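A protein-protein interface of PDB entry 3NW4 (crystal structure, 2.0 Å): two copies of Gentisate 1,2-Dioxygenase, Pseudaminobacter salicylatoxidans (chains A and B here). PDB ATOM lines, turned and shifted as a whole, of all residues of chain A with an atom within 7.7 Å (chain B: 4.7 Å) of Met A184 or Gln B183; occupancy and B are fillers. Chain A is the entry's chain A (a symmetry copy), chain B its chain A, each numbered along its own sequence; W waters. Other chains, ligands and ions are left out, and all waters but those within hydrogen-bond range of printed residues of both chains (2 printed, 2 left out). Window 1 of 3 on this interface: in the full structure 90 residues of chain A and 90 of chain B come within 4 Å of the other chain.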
ATOM      1  N   LEU A  45     -12.286   1.746 -40.218  1.00  0.00           N
ATOM      2  CA  LEU A  45     -11.601   0.974 -39.207  1.00  0.00           C
ATOM      3  C   LEU A  45     -10.141   0.852 -39.553  1.00  0.00           C
ATOM      4  O   LEU A  45      -9.311   0.752 -38.651  1.00  0.00           O
ATOM      5  CB  LEU A  45     -12.216  -0.421 -39.133  1.00  0.00           C
ATOM      6  CG  LEU A  45     -13.094  -0.930 -37.968  1.00  0.00           C
ATOM      7  CD1 LEU A  45     -13.697   0.109 -37.022  1.00  0.00           C
ATOM      8  CD2 LEU A  45     -14.121  -2.014 -38.429  1.00  0.00           C
ATOM      9  N   SER A  52      -6.238  11.023 -37.607  1.00  0.00           N
ATOM     10  CA  SER A  52      -6.698  11.175 -36.252  1.00  0.00           C
ATOM     11  C   SER A  52      -7.990  12.018 -36.180  1.00  0.00           C
ATOM     12  O   SER A  52      -8.222  12.911 -37.028  1.00  0.00           O
ATOM     13  CB  SER A  52      -5.604  11.804 -35.392  1.00  0.00           C
ATOM     14  OG  SER A  52      -6.017  11.830 -34.039  1.00  0.00           O
ATOM     15  N   LYS A  53      -8.817  11.739 -35.163  1.00  0.00           N
ATOM     16  CA  LYS A  53      -9.906  12.654 -34.787  1.00  0.00           C
ATOM     17  C   LYS A  53      -9.360  13.946 -34.148  1.00  0.00           C
ATOM     18  O   LYS A  53      -9.977  15.026 -34.256  1.00  0.00           O
ATOM     19  CB  LYS A  53     -10.858  11.962 -33.828  1.00  0.00           C
ATOM     20  CG  LYS A  53     -11.614  10.801 -34.462  1.00  0.00           C
ATOM     21  CD  LYS A  53     -12.473  10.078 -33.405  1.00  0.00           C
ATOM     22  CE  LYS A  53     -13.144   8.869 -34.029  1.00  0.00           C
ATOM     23  NZ  LYS A  53     -14.099   8.187 -33.068  1.00  0.00           N
ATOM     24  N   LEU A  93     -11.724  15.866 -30.340  1.00  0.00           N
ATOM     25  CA  LEU A  93     -11.863  14.679 -29.467  1.00  0.00           C
ATOM     26  C   LEU A  93     -13.156  14.646 -28.620  1.00  0.00           C
ATOM     27  O   LEU A  93     -13.224  14.023 -27.537  1.00  0.00           O
ATOM     28  CB  LEU A  93     -10.594  14.452 -28.616  1.00  0.00           C
ATOM     29  CG  LEU A  93      -9.345  14.058 -29.424  1.00  0.00           C
ATOM     30  CD1 LEU A  93      -8.138  13.724 -28.496  1.00  0.00           C
ATOM     31  CD2 LEU A  93      -9.626  12.890 -30.343  1.00  0.00           C
ATOM     32  N   TYR A  98      -8.831  15.647 -23.492  1.00  0.00           N
ATOM     33  CA  TYR A  98      -7.636  14.979 -24.026  1.00  0.00           C
ATOM     34  C   TYR A  98      -6.969  15.951 -24.999  1.00  0.00           C
ATOM     35  O   TYR A  98      -7.645  16.406 -25.933  1.00  0.00           O
ATOM     36  CB  TYR A  98      -8.033  13.769 -24.873  1.00  0.00           C
ATOM     37  CG  TYR A  98      -8.790  12.633 -24.225  1.00  0.00           C
ATOM     38  CD1 TYR A  98      -8.954  12.523 -22.834  1.00  0.00           C
ATOM     39  CD2 TYR A  98      -9.311  11.622 -25.033  1.00  0.00           C
ATOM     40  CE1 TYR A  98      -9.626  11.437 -22.282  1.00  0.00           C
ATOM     41  CE2 TYR A  98      -9.955  10.534 -24.499  1.00  0.00           C
ATOM     42  CZ  TYR A  98     -10.120  10.436 -23.142  1.00  0.00           C
ATOM     43  OH  TYR A  98     -10.796   9.328 -22.686  1.00  0.00           O
ATOM     44  N   SER A 100      -4.512  14.870 -26.942  1.00  0.00           N
ATOM     45  CA  SER A 100      -4.360  13.902 -28.026  1.00  0.00           C
ATOM     46  C   SER A 100      -5.047  12.629 -27.522  1.00  0.00           C
ATOM     47  O   SER A 100      -5.476  12.610 -26.359  1.00  0.00           O
ATOM     48  CB  SER A 100      -2.875  13.662 -28.317  1.00  0.00           C
ATOM     49  OG  SER A 100      -2.223  12.880 -27.300  1.00  0.00           O
ATOM     50  N   PRO A 101      -5.135  11.564 -28.367  1.00  0.00           N
ATOM     51  CA  PRO A 101      -5.759  10.312 -27.923  1.00  0.00           C
ATOM     52  C   PRO A 101      -5.037   9.603 -26.775  1.00  0.00           C
ATOM     53  O   PRO A 101      -5.628   8.781 -26.073  1.00  0.00           O
ATOM     54  CB  PRO A 101      -5.733   9.439 -29.190  1.00  0.00           C
ATOM     55  CG  PRO A 101      -5.742  10.480 -30.319  1.00  0.00           C
ATOM     56  CD  PRO A 101      -4.859  11.556 -29.819  1.00  0.00           C
ATOM     57  N   THR A 102      -3.769   9.925 -26.585  1.00  0.00           N
ATOM     58  CA  THR A 102      -2.967   9.289 -25.561  1.00  0.00           C
ATOM     59  C   THR A 102      -2.630  10.197 -24.382  1.00  0.00           C
ATOM     60  O   THR A 102      -2.376   9.695 -23.277  1.00  0.00           O
ATOM     61  CB  THR A 102      -1.638   8.797 -26.145  1.00  0.00           C
ATOM     62  OG1 THR A 102      -0.978   9.890 -26.798  1.00  0.00           O
ATOM     63  CG2 THR A 102      -1.883   7.669 -27.156  1.00  0.00           C
ATOM     64  N   ASP A 177      -0.461  10.377 -18.972  1.00  0.00           N
ATOM     65  CA  ASP A 177      -1.027   9.431 -19.947  1.00  0.00           C
ATOM     66  C   ASP A 177      -2.503   9.120 -19.591  1.00  0.00           C
ATOM     67  O   ASP A 177      -3.019   8.040 -19.897  1.00  0.00           O
ATOM     68  CB  ASP A 177      -0.171   8.146 -20.020  1.00  0.00           C
ATOM     69  CG  ASP A 177       0.023   7.480 -18.644  1.00  0.00           C
ATOM     70  OD1 ASP A 177      -0.767   7.750 -17.713  1.00  0.00           O
ATOM     71  OD2 ASP A 177       0.970   6.700 -18.476  1.00  0.00           O
ATOM     72  N   ILE A 178      -3.187  10.086 -18.960  1.00  0.00           N
ATOM     73  CA  ILE A 178      -4.634   9.972 -18.636  1.00  0.00           C
ATOM     74  C   ILE A 178      -5.558   9.415 -19.771  1.00  0.00           C
ATOM     75  O   ILE A 178      -6.319   8.478 -19.524  1.00  0.00           O
ATOM     76  CB  ILE A 178      -5.183  11.320 -18.023  1.00  0.00           C
ATOM     77  CG1 ILE A 178      -4.794  11.432 -16.528  1.00  0.00           C
ATOM     78  CG2 ILE A 178      -6.721  11.463 -18.200  1.00  0.00           C
ATOM     79  CD1 ILE A 178      -4.994  12.887 -15.958  1.00  0.00           C
ATOM     80  N   PRO A 179      -5.492   9.989 -21.008  1.00  0.00           N
ATOM     81  CA  PRO A 179      -6.405   9.514 -22.079  1.00  0.00           C
ATOM     82  C   PRO A 179      -6.095   8.073 -22.516  1.00  0.00           C
ATOM     83  O   PRO A 179      -7.035   7.295 -22.700  1.00  0.00           O
ATOM     84  CB  PRO A 179      -6.186  10.518 -23.237  1.00  0.00           C
ATOM     85  CG  PRO A 179      -5.615  11.761 -22.541  1.00  0.00           C
ATOM     86  CD  PRO A 179      -4.731  11.180 -21.441  1.00  0.00           C
ATOM     87  N   PHE A 180      -4.823   7.721 -22.680  1.00  0.00           N
ATOM     88  CA  PHE A 180      -4.444   6.312 -22.897  1.00  0.00           C
ATOM     89  C   PHE A 180      -5.006   5.434 -21.786  1.00  0.00           C
ATOM     90  O   PHE A 180      -5.663   4.443 -22.038  1.00  0.00           O
ATOM     91  CB  PHE A 180      -2.905   6.119 -22.978  1.00  0.00           C
ATOM     92  CG  PHE A 180      -2.486   4.685 -23.212  1.00  0.00           C
ATOM     93  CD1 PHE A 180      -2.140   3.863 -22.153  1.00  0.00           C
ATOM     94  CD2 PHE A 180      -2.450   4.152 -24.518  1.00  0.00           C
ATOM     95  CE1 PHE A 180      -1.781   2.520 -22.365  1.00  0.00           C
ATOM     96  CE2 PHE A 180      -2.044   2.871 -24.734  1.00  0.00           C
ATOM     97  CZ  PHE A 180      -1.737   2.025 -23.671  1.00  0.00           C
ATOM     98  N   SER A 181      -4.774   5.826 -20.550  1.00  0.00           N
ATOM     99  CA  SER A 181      -5.153   5.022 -19.414  1.00  0.00           C
ATOM    100  C   SER A 181      -6.660   4.877 -19.226  1.00  0.00           C
ATOM    101  O   SER A 181      -7.139   3.810 -18.848  1.00  0.00           O
ATOM    102  CB  SER A 181      -4.529   5.643 -18.164  1.00  0.00           C
ATOM    103  OG  SER A 181      -3.092   5.489 -18.213  1.00  0.00           O
ATOM    104  N   GLN A 182      -7.398   5.963 -19.444  1.00  0.00           N
ATOM    105  CA  GLN A 182      -8.848   5.882 -19.430  1.00  0.00           C
ATOM    106  C   GLN A 182      -9.379   4.984 -20.542  1.00  0.00           C
ATOM    107  O   GLN A 182     -10.212   4.123 -20.297  1.00  0.00           O
ATOM    108  CB  GLN A 182      -9.505   7.272 -19.545  1.00  0.00           C
ATOM    109  CG  GLN A 182     -11.050   7.146 -19.501  1.00  0.00           C
ATOM    110  CD  GLN A 182     -11.752   8.447 -19.333  1.00  0.00           C
ATOM    111  OE1 GLN A 182     -12.595   8.576 -18.440  1.00  0.00           O
ATOM    112  NE2 GLN A 182     -11.469   9.412 -20.210  1.00  0.00           N
ATOM    113  N   GLN A 183      -8.930   5.183 -21.775  1.00  0.00           N
ATOM    114  CA  GLN A 183      -9.473   4.326 -22.851  1.00  0.00           C
ATOM    115  C   GLN A 183      -9.065   2.854 -22.757  1.00  0.00           C
ATOM    116  O   GLN A 183      -9.840   1.969 -23.187  1.00  0.00           O
ATOM    117  CB  GLN A 183      -9.083   4.886 -24.229  1.00  0.00           C
ATOM    118  CG  GLN A 183      -9.810   6.187 -24.602  1.00  0.00           C
ATOM    119  CD  GLN A 183      -9.039   6.986 -25.696  1.00  0.00           C
ATOM    120  OE1 GLN A 183      -7.896   7.369 -25.507  1.00  0.00           O
ATOM    121  NE2 GLN A 183      -9.685   7.242 -26.809  1.00  0.00           N
ATOM    122  N   MET A 184      -7.863   2.567 -22.260  1.00  0.00           N
ATOM    123  CA  MET A 184      -7.332   1.186 -22.215  1.00  0.00           C
ATOM    124  C   MET A 184      -7.672   0.432 -20.910  1.00  0.00           C
ATOM    125  O   MET A 184      -7.361  -0.772 -20.780  1.00  0.00           O
ATOM    126  CB  MET A 184      -5.806   1.211 -22.395  1.00  0.00           C
ATOM    127  CG  MET A 184      -5.373   1.824 -23.736  1.00  0.00           C
ATOM    128  SD  MET A 184      -6.065   0.861 -25.096  1.00  0.00           S
ATOM    129  CE  MET A 184      -7.488   1.622 -25.659  1.00  0.00           C
ATOM    130  N   ASP A 185      -8.217   1.173 -19.938  1.00  0.00           N
ATOM    131  CA  ASP A 185      -8.703   0.638 -18.632  1.00  0.00           C
ATOM    132  C   ASP A 185      -7.568   0.172 -17.722  1.00  0.00           C
ATOM    133  O   ASP A 185      -7.591  -0.945 -17.247  1.00  0.00           O
ATOM    134  CB  ASP A 185      -9.712  -0.524 -18.849  1.00  0.00           C
ATOM    135  CG  ASP A 185     -10.991  -0.093 -19.584  1.00  0.00           C
ATOM    136  OD1 ASP A 185     -11.535   1.005 -19.302  1.00  0.00           O
ATOM    137  OD2 ASP A 185     -11.495  -0.896 -20.410  1.00  0.00           O
ATOM    138  N   VAL A 186      -6.580   1.029 -17.459  1.00  0.00           N
ATOM    139  CA  VAL A 186      -5.458   0.651 -16.618  1.00  0.00           C
ATOM    140  C   VAL A 186      -5.341   1.537 -15.353  1.00  0.00           C
ATOM    141  O   VAL A 186      -4.396   1.397 -14.596  1.00  0.00           O
ATOM    142  CB  VAL A 186      -4.118   0.675 -17.409  1.00  0.00           C
ATOM    143  CG1 VAL A 186      -4.177  -0.247 -18.645  1.00  0.00           C
ATOM    144  CG2 VAL A 186      -3.774   2.116 -17.851  1.00  0.00           C
ATOM    145  N   GLY A 187      -6.322   2.415 -15.151  1.00  0.00           N
ATOM    146  CA  GLY A 187      -6.306   3.389 -14.066  1.00  0.00           C
ATOM    147  C   GLY A 187      -6.638   2.805 -12.710  1.00  0.00           C
ATOM    148  O   GLY A 187      -7.664   2.165 -12.534  1.00  0.00           O
ATOM    149  N   ILE A 353       5.151   4.332 -26.353  1.00  0.00           N
ATOM    150  CA  ILE A 353       4.073   3.361 -26.651  1.00  0.00           C
ATOM    151  C   ILE A 353       4.198   2.772 -28.077  1.00  0.00           C
ATOM    152  O   ILE A 353       4.137   1.543 -28.267  1.00  0.00           O
ATOM    153  CB  ILE A 353       2.643   3.951 -26.460  1.00  0.00           C
ATOM    154  CG1 ILE A 353       2.464   4.464 -25.006  1.00  0.00           C
ATOM    155  CG2 ILE A 353       1.565   2.905 -26.865  1.00  0.00           C
ATOM    156  CD1 ILE A 353       1.119   5.160 -24.725  1.00  0.00           C
ATOM    157  N   MET A 354       4.378   3.651 -29.057  1.00  0.00           N
ATOM    158  CA  MET A 354       4.394   3.268 -30.458  1.00  0.00           C
ATOM    159  C   MET A 354       5.589   2.353 -30.745  1.00  0.00           C
ATOM    160  O   MET A 354       5.454   1.353 -31.451  1.00  0.00           O
ATOM    161  CB  MET A 354       4.466   4.520 -31.345  1.00  0.00           C
ATOM    162  CG  MET A 354       3.378   5.584 -30.995  1.00  0.00           C
ATOM    163  SD  MET A 354       1.772   4.827 -31.100  1.00  0.00           S
ATOM    164  CE  MET A 354       0.702   5.979 -30.241  1.00  0.00           C
ATOM    165  N   TYR B  98     -16.168  -3.074 -31.592  1.00  0.00           N
ATOM    166  CA  TYR B  98     -15.042  -3.458 -30.728  1.00  0.00           C
ATOM    167  C   TYR B  98     -15.566  -4.495 -29.734  1.00  0.00           C
ATOM    168  O   TYR B  98     -16.546  -4.199 -29.035  1.00  0.00           O
ATOM    169  CB  TYR B  98     -14.594  -2.271 -29.874  1.00  0.00           C
ATOM    170  CG  TYR B  98     -14.082  -1.024 -30.556  1.00  0.00           C
ATOM    171  CD1 TYR B  98     -13.782  -0.977 -31.928  1.00  0.00           C
ATOM    172  CD2 TYR B  98     -13.851   0.118 -29.789  1.00  0.00           C
ATOM    173  CE1 TYR B  98     -13.275   0.185 -32.503  1.00  0.00           C
ATOM    174  CE2 TYR B  98     -13.329   1.262 -30.340  1.00  0.00           C
ATOM    175  CZ  TYR B  98     -13.046   1.306 -31.680  1.00  0.00           C
ATOM    176  OH  TYR B  98     -12.548   2.494 -32.163  1.00  0.00           O
ATOM    177  N   PRO B 101     -11.942  -2.582 -25.591  1.00  0.00           N
ATOM    178  CA  PRO B 101     -11.308  -1.336 -26.033  1.00  0.00           C
ATOM    179  C   PRO B 101     -10.061  -1.519 -26.902  1.00  0.00           C
ATOM    180  O   PRO B 101      -9.663  -0.609 -27.631  1.00  0.00           O
ATOM    181  CB  PRO B 101     -10.939  -0.641 -24.711  1.00  0.00           C
ATOM    182  CG  PRO B 101     -11.977  -1.208 -23.730  1.00  0.00           C
ATOM    183  CD  PRO B 101     -12.099  -2.629 -24.122  1.00  0.00           C
ATOM    184  N   THR B 102      -9.455  -2.691 -26.825  1.00  0.00           N
ATOM    185  CA  THR B 102      -8.239  -2.969 -27.563  1.00  0.00           C
ATOM    186  C   THR B 102      -8.425  -3.946 -28.721  1.00  0.00           C
ATOM    187  O   THR B 102      -7.638  -3.916 -29.678  1.00  0.00           O
ATOM    188  CB  THR B 102      -7.171  -3.564 -26.639  1.00  0.00           C
ATOM    189  OG1 THR B 102      -7.715  -4.710 -25.969  1.00  0.00           O
ATOM    190  CG2 THR B 102      -6.726  -2.527 -25.599  1.00  0.00           C
ATOM    191  N   PRO B 179      -9.297  -2.045 -32.625  1.00  0.00           N
ATOM    192  CA  PRO B 179      -9.771  -0.941 -31.751  1.00  0.00           C
ATOM    193  C   PRO B 179      -8.610  -0.167 -31.105  1.00  0.00           C
ATOM    194  O   PRO B 179      -8.671   1.065 -31.063  1.00  0.00           O
ATOM    195  CB  PRO B 179     -10.644  -1.648 -30.685  1.00  0.00           C
ATOM    196  CG  PRO B 179     -11.041  -2.970 -31.357  1.00  0.00           C
ATOM    197  CD  PRO B 179      -9.798  -3.354 -32.155  1.00  0.00           C
ATOM    198  N   PHE B 180      -7.585  -0.856 -30.615  1.00  0.00           N
ATOM    199  CA  PHE B 180      -6.353  -0.178 -30.169  1.00  0.00           C
ATOM    200  C   PHE B 180      -5.801   0.705 -31.281  1.00  0.00           C
ATOM    201  O   PHE B 180      -5.541   1.876 -31.086  1.00  0.00           O
ATOM    202  CB  PHE B 180      -5.257  -1.179 -29.714  1.00  0.00           C
ATOM    203  CG  PHE B 180      -3.986  -0.512 -29.239  1.00  0.00           C
ATOM    204  CD1 PHE B 180      -2.914  -0.333 -30.097  1.00  0.00           C
ATOM    205  CD2 PHE B 180      -3.871  -0.046 -27.913  1.00  0.00           C
ATOM    206  CE1 PHE B 180      -1.742   0.317 -29.667  1.00  0.00           C
ATOM    207  CE2 PHE B 180      -2.717   0.527 -27.474  1.00  0.00           C
ATOM    208  CZ  PHE B 180      -1.651   0.751 -28.343  1.00  0.00           C
ATOM    209  N   SER B 181      -5.659   0.143 -32.464  1.00  0.00           N
ATOM    210  CA  SER B 181      -5.040   0.838 -33.566  1.00  0.00           C
ATOM    211  C   SER B 181      -5.841   2.030 -34.082  1.00  0.00           C
ATOM    212  O   SER B 181      -5.266   3.054 -34.447  1.00  0.00           O
ATOM    213  CB  SER B 181      -4.815  -0.168 -34.696  1.00  0.00           C
ATOM    214  OG  SER B 181      -3.804  -1.123 -34.299  1.00  0.00           O
ATOM    215  N   GLN B 182      -7.161   1.877 -34.156  1.00  0.00           N
ATOM    216  CA  GLN B 182      -8.014   3.002 -34.498  1.00  0.00           C
ATOM    217  C   GLN B 182      -7.942   4.108 -33.451  1.00  0.00           C
ATOM    218  O   GLN B 182      -7.775   5.271 -33.791  1.00  0.00           O
ATOM    219  CB  GLN B 182      -9.484   2.575 -34.684  1.00  0.00           C
ATOM    220  CG  GLN B 182     -10.356   3.798 -35.072  1.00  0.00           C
ATOM    221  CD  GLN B 182     -11.724   3.435 -35.534  1.00  0.00           C
ATOM    222  OE1 GLN B 182     -12.144   3.879 -36.606  1.00  0.00           O
ATOM    223  NE2 GLN B 182     -12.462   2.677 -34.721  1.00  0.00           N
ATOM    224  N   GLN B 183      -8.091   3.774 -32.175  1.00  0.00           N
ATOM    225  CA  GLN B 183      -8.051   4.857 -31.170  1.00  0.00           C
ATOM    226  C   GLN B 183      -6.682   5.525 -31.012  1.00  0.00           C
ATOM    227  O   GLN B 183      -6.616   6.731 -30.683  1.00  0.00           O
ATOM    228  CB  GLN B 183      -8.538   4.342 -29.807  1.00  0.00           C
ATOM    229  CG  GLN B 183     -10.046   4.054 -29.750  1.00  0.00           C
ATOM    230  CD  GLN B 183     -10.403   3.067 -28.598  1.00  0.00           C
ATOM    231  OE1 GLN B 183      -9.921   1.947 -28.556  1.00  0.00           O
ATOM    232  NE2 GLN B 183     -11.258   3.492 -27.698  1.00  0.00           N
ATOM    233  N   MET B 184      -5.596   4.774 -31.184  1.00  0.00           N
ATOM    234  CA  MET B 184      -4.228   5.294 -30.959  1.00  0.00           C
ATOM    235  C   MET B 184      -3.582   5.909 -32.221  1.00  0.00           C
ATOM    236  O   MET B 184      -2.465   6.466 -32.148  1.00  0.00           O
ATOM    237  CB  MET B 184      -3.324   4.167 -30.434  1.00  0.00           C
ATOM    238  CG  MET B 184      -3.815   3.581 -29.101  1.00  0.00           C
ATOM    239  SD  MET B 184      -3.855   4.875 -27.845  1.00  0.00           S
ATOM    240  CE  MET B 184      -5.447   5.481 -27.711  1.00  0.00           C
ATOM    241  N   ASP B 185      -4.250   5.719 -33.365  1.00  0.00           N
ATOM    242  CA  ASP B 185      -3.858   6.296 -34.685  1.00  0.00           C
ATOM    243  C   ASP B 185      -2.585   5.671 -35.253  1.00  0.00           C
ATOM    244  O   ASP B 185      -1.664   6.380 -35.600  1.00  0.00           O
ATOM    245  CB  ASP B 185      -3.686   7.837 -34.586  1.00  0.00           C
ATOM    246  CG  ASP B 185      -4.983   8.574 -34.217  1.00  0.00           C
ATOM    247  OD1 ASP B 185      -6.073   8.218 -34.732  1.00  0.00           O
ATOM    248  OD2 ASP B 185      -4.899   9.568 -33.451  1.00  0.00           O
ATOM    249  N   MET B 354      -0.239  -4.287 -21.888  1.00  0.00           N
ATOM    250  CA  MET B 354      -0.271  -3.898 -20.488  1.00  0.00           C
ATOM    251  C   MET B 354       1.095  -4.143 -19.838  1.00  0.00           C
ATOM    252  O   MET B 354       1.585  -3.305 -19.081  1.00  0.00           O
ATOM    253  CB  MET B 354      -1.357  -4.690 -19.746  1.00  0.00           C
ATOM    254  CG  MET B 354      -2.750  -4.629 -20.448  1.00  0.00           C
ATOM    255  SD  MET B 354      -3.229  -2.927 -20.639  1.00  0.00           S
ATOM    256  CE  MET B 354      -4.558  -2.992 -21.839  1.00  0.00           C
HETATM  257  O   HOH W   1      -8.308   9.453 -33.446  1.00  0.00           O
HETATM  258  O   HOH W   2      -7.835  -0.121 -36.581  1.00  0.00           O
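Of the 21 printed residues of chain A, 10 touch a printed residue of chain B.
Hydrophobic or aromatic side chains of chain A within 4 Å of the printed part of chain B: Leu A45, Pro A101, Phe A180, Met A184, Val A186 and Met A354.
The side-chain carboxylate (OD2) of Asp B185 sits at hydrogen-bond distance from the side-chain hydroxyl (OG) of Ser A52 (2.6 Å).
Met A184 touches just these residues of chain B: Pro B101, Thr B102, Phe B180, Gln B183 and Met B354.
Printed residues of chain B within 4 Å of Met A354: Met B184.
Of chain A, only Pro A101 (3.2 Å) and Met A184 (3.8 Å) come within 4 Å of Gln B183.
Printed residues of chain A within 4 Å of Met B354: Met A184 and Val A186.
The nearest printed residue of chain B that does not touch Met A184 is Met B184 (4.8 Å).
The nearest residue of chain A that does not touch Gln B183 is Gln A183 (4.2 Å).
The nearest printed residue of chain A that does not touch Met B354 is Asp A185 (5.9 Å).
Among the printed residues, pairs that only touch across the chains: Leu A45 with Gln B182 (3.7 Å), Pro A101 with Gln B183 (3.2 Å), Pro A101 with Met B184 (3.7 Å), Pro A101 with Asp B185 (3.4 Å), Thr A102 with Met B184 (3.5 Å), Phe A180 with Phe B180 (3.7 Å), Phe A180 with Met B184 (3.7 Å), Gln A183 with Pro B101 (3.2 Å), Gln A183 with Met B184 (3.8 Å), Met A184 with Pro B101 (3.7 Å), Met A184 with Thr B102 (3.5 Å), Met A184 with Phe B180 (3.7 Å), Met A184 with Gln B183 (3.8 Å), Met A184 with Met B354 (3.7 Å), Asp A185 with Pro B101 (3.4 Å), Val A186 with Met B354 (3.5 Å) and Met A354 with Met B184 (3.7 Å).
Pro A101 touches Gln B183, and with the chains exchanged Gln A183 touches Pro B101.
Pro A101 touches Asp B185, and with the chains exchanged Asp A185 touches Pro B101.
Thr A102 touches Met B184, and with the chains exchanged Met A184 touches Thr B102.
Phe B180 touches its own counterpart, Phe A180.
Water W2 lies within hydrogen-bond range of the backbone carbonyl oxygen of Leu A45 and the backbone NH of Gln B182.
Water W1 lies within hydrogen-bond range of the side-chain carboxylate of Asp B185 (2.9 Å), the backbone NH of Lys A53 (2.9 Å) and the side-chain hydroxyl of Ser A52 (3.4 Å).
The side-chain amide nitrogen of Gln B182 sits at hydrogen-bond distance from the side-chain hydroxyl of Tyr B98 (2.6 Å).
The backbone carbonyl oxygen (O) of Pro A101 lies close to the side-chain amide oxygen (OE1) of Gln A183, at 2.7 Å.
The backbone NH (N) of Phe A180 sits at hydrogen-bond distance from the backbone carbonyl oxygen (O) of Thr A102 (3.2 Å).
The side-chain hydroxyl of Thr A102 sits at hydrogen-bond distance from the side-chain hydroxyl of Ser A100, at 3.3 Å.
The side-chain amide oxygen of Gln B183 sits close to the backbone carbonyl oxygen of Pro B179 (2.9 Å).
O of Ser A181 sits at hydrogen-bond distance from N of Val A186, 3.2 Å away.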
